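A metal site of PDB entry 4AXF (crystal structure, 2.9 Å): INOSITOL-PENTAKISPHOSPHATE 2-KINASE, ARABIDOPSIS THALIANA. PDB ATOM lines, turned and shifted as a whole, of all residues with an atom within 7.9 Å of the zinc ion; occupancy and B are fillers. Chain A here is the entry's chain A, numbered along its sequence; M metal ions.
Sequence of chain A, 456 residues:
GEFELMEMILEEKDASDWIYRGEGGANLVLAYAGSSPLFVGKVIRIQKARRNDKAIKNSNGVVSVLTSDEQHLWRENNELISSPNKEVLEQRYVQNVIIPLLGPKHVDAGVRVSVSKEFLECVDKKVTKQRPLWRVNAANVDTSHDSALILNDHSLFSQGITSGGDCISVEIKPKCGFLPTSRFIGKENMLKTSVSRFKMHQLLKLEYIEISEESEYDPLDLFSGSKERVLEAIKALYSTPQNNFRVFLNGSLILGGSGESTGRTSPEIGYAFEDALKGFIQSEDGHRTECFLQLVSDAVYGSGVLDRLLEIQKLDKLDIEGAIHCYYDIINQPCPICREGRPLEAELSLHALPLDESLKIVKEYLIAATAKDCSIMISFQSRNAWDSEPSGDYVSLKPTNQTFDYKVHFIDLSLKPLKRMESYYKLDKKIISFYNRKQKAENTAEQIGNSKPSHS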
ATOM      1  N   GLU A 321      12.530  -1.289 -24.356  1.00  0.00           N
ATOM      2  CA  GLU A 321      13.173  -2.607 -24.397  1.00  0.00           C
ATOM      3  C   GLU A 321      13.894  -2.943 -23.106  1.00  0.00           C
ATOM      4  O   GLU A 321      14.175  -4.108 -22.831  1.00  0.00           O
ATOM      5  CB  GLU A 321      14.128  -2.726 -25.578  1.00  0.00           C
ATOM      6  CG  GLU A 321      13.430  -2.983 -26.906  1.00  0.00           C
ATOM      7  CD  GLU A 321      14.389  -3.452 -27.985  1.00  0.00           C
ATOM      8  OE1 GLU A 321      14.762  -4.644 -27.981  1.00  0.00           O
ATOM      9  OE2 GLU A 321      14.763  -2.628 -28.828  1.00  0.00           O
ATOM     10  N   GLY A 322      14.175  -1.919 -22.309  1.00  0.00           N
ATOM     11  CA  GLY A 322      14.703  -2.115 -20.967  1.00  0.00           C
ATOM     12  C   GLY A 322      13.586  -2.115 -19.948  1.00  0.00           C
ATOM     13  O   GLY A 322      13.469  -3.048 -19.142  1.00  0.00           O
ATOM     14  N   ILE A 324      10.424  -2.628 -20.098  1.00  0.00           N
ATOM     15  CA  ILE A 324       9.430  -3.698 -20.192  1.00  0.00           C
ATOM     16  C   ILE A 324       9.682  -4.809 -19.172  1.00  0.00           C
ATOM     17  O   ILE A 324       8.733  -5.346 -18.594  1.00  0.00           O
ATOM     18  CB  ILE A 324       9.302  -4.263 -21.632  1.00  0.00           C
ATOM     19  CG1 ILE A 324       8.067  -5.162 -21.775  1.00  0.00           C
ATOM     20  CG2 ILE A 324      10.564  -5.004 -22.065  1.00  0.00           C
ATOM     21  CD1 ILE A 324       6.760  -4.412 -21.701  1.00  0.00           C
ATOM     22  N   HIS A 325      10.958  -5.121 -18.937  1.00  0.00           N
ATOM     23  CA  HIS A 325      11.336  -6.185 -18.006  1.00  0.00           C
ATOM     24  C   HIS A 325      10.974  -5.817 -16.588  1.00  0.00           C
ATOM     25  O   HIS A 325      10.547  -6.675 -15.820  1.00  0.00           O
ATOM     26  CB  HIS A 325      12.830  -6.488 -18.120  1.00  0.00           C
ATOM     27  CG  HIS A 325      13.253  -6.935 -19.504  1.00  0.00           C
ATOM     28  ND1 HIS A 325      13.277  -8.227 -19.868  1.00  0.00           N
ATOM     29  CD2 HIS A 325      13.661  -6.198 -20.620  1.00  0.00           C
ATOM     30  CE1 HIS A 325      13.686  -8.323 -21.157  1.00  0.00           C
ATOM     31  NE2 HIS A 325      13.920  -7.079 -21.612  1.00  0.00           N
ATOM     32  N   CYS A 326      11.122  -4.538 -16.249  1.00  0.00           N
ATOM     33  CA  CYS A 326      10.751  -4.021 -14.934  1.00  0.00           C
ATOM     34  C   CYS A 326       9.228  -4.028 -14.718  1.00  0.00           C
ATOM     35  O   CYS A 326       8.762  -4.224 -13.590  1.00  0.00           O
ATOM     36  CB  CYS A 326      11.289  -2.614 -14.734  1.00  0.00           C
ATOM     37  SG  CYS A 326      13.089  -2.480 -14.796  1.00  0.00           S
ATOM     38  N   TYR A 328       7.068  -6.286 -15.840  1.00  0.00           N
ATOM     39  CA  TYR A 328       6.684  -7.643 -15.460  1.00  0.00           C
ATOM     40  C   TYR A 328       7.113  -7.996 -14.038  1.00  0.00           C
ATOM     41  O   TYR A 328       6.517  -8.873 -13.403  1.00  0.00           O
ATOM     42  CB  TYR A 328       7.207  -8.669 -16.468  1.00  0.00           C
ATOM     43  CG  TYR A 328       6.521  -8.570 -17.821  1.00  0.00           C
ATOM     44  CD1 TYR A 328       5.194  -8.993 -17.986  1.00  0.00           C
ATOM     45  CD2 TYR A 328       7.186  -8.058 -18.930  1.00  0.00           C
ATOM     46  CE1 TYR A 328       4.563  -8.895 -19.210  1.00  0.00           C
ATOM     47  CE2 TYR A 328       6.559  -7.959 -20.162  1.00  0.00           C
ATOM     48  CZ  TYR A 328       5.251  -8.380 -20.295  1.00  0.00           C
ATOM     49  OH  TYR A 328       4.632  -8.277 -21.524  1.00  0.00           O
ATOM     50  N   ASP A 329       8.142  -7.311 -13.548  1.00  0.00           N
ATOM     51  CA  ASP A 329       8.573  -7.456 -12.149  1.00  0.00           C
ATOM     52  C   ASP A 329       7.612  -6.741 -11.215  1.00  0.00           C
ATOM     53  O   ASP A 329       7.407  -7.170 -10.078  1.00  0.00           O
ATOM     54  CB  ASP A 329       9.986  -6.912 -11.961  1.00  0.00           C
ATOM     55  CG  ASP A 329      11.068  -7.901 -12.377  1.00  0.00           C
ATOM     56  OD1 ASP A 329      10.755  -9.092 -12.575  1.00  0.00           O
ATOM     57  OD2 ASP A 329      12.236  -7.487 -12.484  1.00  0.00           O
ATOM     58  N   GLN A 333       4.377 -10.852 -12.617  1.00  0.00           N
ATOM     59  CA  GLN A 333       4.161 -11.826 -13.668  1.00  0.00           C
ATOM     60  C   GLN A 333       5.496 -12.297 -14.241  1.00  0.00           C
ATOM     61  O   GLN A 333       6.410 -11.491 -14.428  1.00  0.00           O
ATOM     62  CB  GLN A 333       3.271 -11.241 -14.762  1.00  0.00           C
ATOM     63  CG  GLN A 333       2.539 -12.280 -15.598  1.00  0.00           C
ATOM     64  CD  GLN A 333       2.058 -11.729 -16.937  1.00  0.00           C
ATOM     65  OE1 GLN A 333       1.306 -10.750 -16.985  1.00  0.00           O
ATOM     66  NE2 GLN A 333       2.501 -12.359 -18.024  1.00  0.00           N
ATOM     67  N   PRO A 334       5.631 -13.614 -14.507  1.00  0.00           N
ATOM     68  CA  PRO A 334       6.798 -14.138 -15.226  1.00  0.00           C
ATOM     69  C   PRO A 334       7.008 -13.387 -16.543  1.00  0.00           C
ATOM     70  O   PRO A 334       6.044 -13.154 -17.281  1.00  0.00           O
ATOM     71  CB  PRO A 334       6.399 -15.590 -15.495  1.00  0.00           C
ATOM     72  CG  PRO A 334       5.518 -15.942 -14.357  1.00  0.00           C
ATOM     73  CD  PRO A 334       4.770 -14.695 -13.993  1.00  0.00           C
ATOM     74  N   CYS A 335       8.260 -13.024 -16.816  1.00  0.00           N
ATOM     75  CA  CYS A 335       8.604 -12.212 -17.979  1.00  0.00           C
ATOM     76  C   CYS A 335       8.582 -13.030 -19.277  1.00  0.00           C
ATOM     77  O   CYS A 335       9.331 -14.001 -19.410  1.00  0.00           O
ATOM     78  CB  CYS A 335       9.971 -11.544 -17.781  1.00  0.00           C
ATOM     79  SG  CYS A 335      10.498 -10.424 -19.090  1.00  0.00           S
ATOM     80  N   PRO A 336       7.729 -12.632 -20.235  1.00  0.00           N
ATOM     81  CA  PRO A 336       7.632 -13.275 -21.542  1.00  0.00           C
ATOM     82  C   PRO A 336       8.880 -13.024 -22.380  1.00  0.00           C
ATOM     83  O   PRO A 336       9.452 -13.965 -22.926  1.00  0.00           O
ATOM     84  CB  PRO A 336       6.416 -12.593 -22.195  1.00  0.00           C
ATOM     85  CG  PRO A 336       5.697 -11.888 -21.094  1.00  0.00           C
ATOM     86  CD  PRO A 336       6.771 -11.526 -20.106  1.00  0.00           C
ATOM     87  N   ILE A 337       9.295 -11.756 -22.460  1.00  0.00           N
ATOM     88  CA  ILE A 337      10.445 -11.334 -23.263  1.00  0.00           C
ATOM     89  C   ILE A 337      11.689 -12.173 -22.962  1.00  0.00           C
ATOM     90  O   ILE A 337      12.403 -12.589 -23.879  1.00  0.00           O
ATOM     91  CB  ILE A 337      10.785  -9.838 -23.043  1.00  0.00           C
ATOM     92  CG1 ILE A 337       9.547  -8.992 -22.732  1.00  0.00           C
ATOM     93  CG2 ILE A 337      11.584  -9.286 -24.226  1.00  0.00           C
ATOM     94  CD1 ILE A 337       8.538  -8.855 -23.863  1.00  0.00           C
ATOM     95  N   CYS A 338      11.952 -12.423 -21.681  1.00  0.00           N
ATOM     96  CA  CYS A 338      13.107 -13.207 -21.251  1.00  0.00           C
ATOM     97  C   CYS A 338      12.968 -14.700 -21.560  1.00  0.00           C
ATOM     98  O   CYS A 338      13.826 -15.281 -22.217  1.00  0.00           O
ATOM     99  CB  CYS A 338      13.377 -13.014 -19.753  1.00  0.00           C
ATOM    100  SG  CYS A 338      14.081 -11.412 -19.337  1.00  0.00           S
ATOM    101  N   ARG A 339      11.878 -15.306 -21.093  1.00  0.00           N
ATOM    102  CA  ARG A 339      11.703 -16.765 -21.192  1.00  0.00           C
ATOM    103  C   ARG A 339      11.239 -17.284 -22.550  1.00  0.00           C
ATOM    104  O   ARG A 339      11.422 -18.461 -22.856  1.00  0.00           O
ATOM    105  CB  ARG A 339      10.813 -17.300 -20.065  1.00  0.00           C
ATOM    106  CG  ARG A 339      11.528 -18.252 -19.121  1.00  0.00           C
ATOM    107  CD  ARG A 339      10.574 -18.865 -18.101  1.00  0.00           C
ATOM    108  NE  ARG A 339      10.249 -17.926 -17.024  1.00  0.00           N
ATOM    109  CZ  ARG A 339       9.557 -18.230 -15.931  1.00  0.00           C
ATOM    110  NH1 ARG A 339       9.104 -19.468 -15.744  1.00  0.00           N
ATOM    111  NH2 ARG A 339       9.327 -17.293 -15.020  1.00  0.00           N
ATOM    112  N   GLU A 345      20.500 -14.630 -23.510  1.00  0.00           N
ATOM    113  CA  GLU A 345      20.328 -13.201 -23.759  1.00  0.00           C
ATOM    114  C   GLU A 345      19.299 -12.572 -22.823  1.00  0.00           C
ATOM    115  O   GLU A 345      18.860 -11.439 -23.035  1.00  0.00           O
ATOM    116  CB  GLU A 345      19.915 -12.956 -25.218  1.00  0.00           C
ATOM    117  CG  GLU A 345      21.019 -13.204 -26.224  1.00  0.00           C
ATOM    118  CD  GLU A 345      20.549 -13.038 -27.663  1.00  0.00           C
ATOM    119  OE1 GLU A 345      19.420 -12.533 -27.872  1.00  0.00           O
ATOM    120  OE2 GLU A 345      21.307 -13.422 -28.577  1.00  0.00           O
ATOM    121  N   ALA A 346      18.928 -13.314 -21.791  1.00  0.00           N
ATOM    122  CA  ALA A 346      17.967 -12.866 -20.782  1.00  0.00           C
ATOM    123  C   ALA A 346      18.548 -11.722 -19.956  1.00  0.00           C
ATOM    124  O   ALA A 346      19.695 -11.786 -19.502  1.00  0.00           O
ATOM    125  CB  ALA A 346      17.555 -14.011 -19.878  1.00  0.00           C
ATOM    126  N   GLU A 347      17.755 -10.665 -19.781  1.00  0.00           N
ATOM    127  CA  GLU A 347      18.196  -9.475 -19.044  1.00  0.00           C
ATOM    128  C   GLU A 347      18.181  -9.710 -17.531  1.00  0.00           C
ATOM    129  O   GLU A 347      17.321  -9.189 -16.814  1.00  0.00           O
ATOM    130  CB  GLU A 347      17.347  -8.243 -19.432  1.00  0.00           C
ATOM    131  CG  GLU A 347      17.319  -7.926 -20.924  1.00  0.00           C
ATOM    132  CD  GLU A 347      18.582  -7.258 -21.443  1.00  0.00           C
ATOM    133  OE1 GLU A 347      19.564  -7.134 -20.672  1.00  0.00           O
ATOM    134  OE2 GLU A 347      18.598  -6.855 -22.622  1.00  0.00           O
ATOM    135  N   LEU A 348      19.163 -10.493 -17.065  1.00  0.00           N
ATOM    136  CA  LEU A 348      19.354 -10.801 -15.647  1.00  0.00           C
ATOM    137  C   LEU A 348      19.615  -9.529 -14.847  1.00  0.00           C
ATOM    138  O   LEU A 348      19.079  -9.351 -13.750  1.00  0.00           O
ATOM    139  CB  LEU A 348      20.516 -11.783 -15.468  1.00  0.00           C
ATOM    140  CG  LEU A 348      20.311 -13.314 -15.511  1.00  0.00           C
ATOM    141  CD1 LEU A 348      19.528 -13.795 -16.723  1.00  0.00           C
ATOM    142  CD2 LEU A 348      21.658 -14.014 -15.436  1.00  0.00           C
ATOM    143  N   LEU A 350      18.435  -6.512 -15.090  1.00  0.00           N
ATOM    144  CA  LEU A 350      17.236  -5.780 -14.693  1.00  0.00           C
ATOM    145  C   LEU A 350      16.396  -6.491 -13.647  1.00  0.00           C
ATOM    146  O   LEU A 350      15.911  -5.867 -12.706  1.00  0.00           O
ATOM    147  CB  LEU A 350      16.377  -5.455 -15.931  1.00  0.00           C
ATOM    148  CG  LEU A 350      16.926  -4.414 -16.911  1.00  0.00           C
ATOM    149  CD1 LEU A 350      16.260  -4.550 -18.277  1.00  0.00           C
ATOM    150  CD2 LEU A 350      16.760  -2.997 -16.370  1.00  0.00           C
ATOM    151  N   HIS A 351      16.239  -7.805 -13.802  1.00  0.00           N
ATOM    152  CA  HIS A 351      15.416  -8.594 -12.891  1.00  0.00           C
ATOM    153  C   HIS A 351      16.024  -8.760 -11.517  1.00  0.00           C
ATOM    154  O   HIS A 351      15.327  -9.085 -10.552  1.00  0.00           O
ATOM    155  CB  HIS A 351      15.065  -9.938 -13.508  1.00  0.00           C
ATOM    156  CG  HIS A 351      14.092  -9.833 -14.669  1.00  0.00           C
ATOM    157  ND1 HIS A 351      12.795  -9.542 -14.488  1.00  0.00           N
ATOM    158  CD2 HIS A 351      14.284  -9.995 -16.028  1.00  0.00           C
ATOM    159  CE1 HIS A 351      12.175  -9.523 -15.680  1.00  0.00           C
ATOM    160  NE2 HIS A 351      13.085  -9.797 -16.630  1.00  0.00           N
HETATM  161 ZN    ZN M   1      12.609  -9.961 -18.759  1.00  0.00          ZN
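The side-chain sulfur (SG) of Cys 338 sits close to the backbone NH (N) of Glu 347, at 3.8 Å. A ring nitrogen (NE2) of His 325 lies close to the backbone carbonyl oxygen (O) of Glu 321. A ring nitrogen (ND1) of His 351 sits at hydrogen-bond distance from the side-chain carboxylate of Asp 329, at 2.8 Å.
Of the 20 residues printed, 4 come within 4 Å of the zinc ion. Along chain A the residues within 4 Å of the zinc ion span positions 325 to 351.
The zinc ion is bound by SG of Cys 338, ND1 of His 325, SG of Cys 335 and NE2 of His 351.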
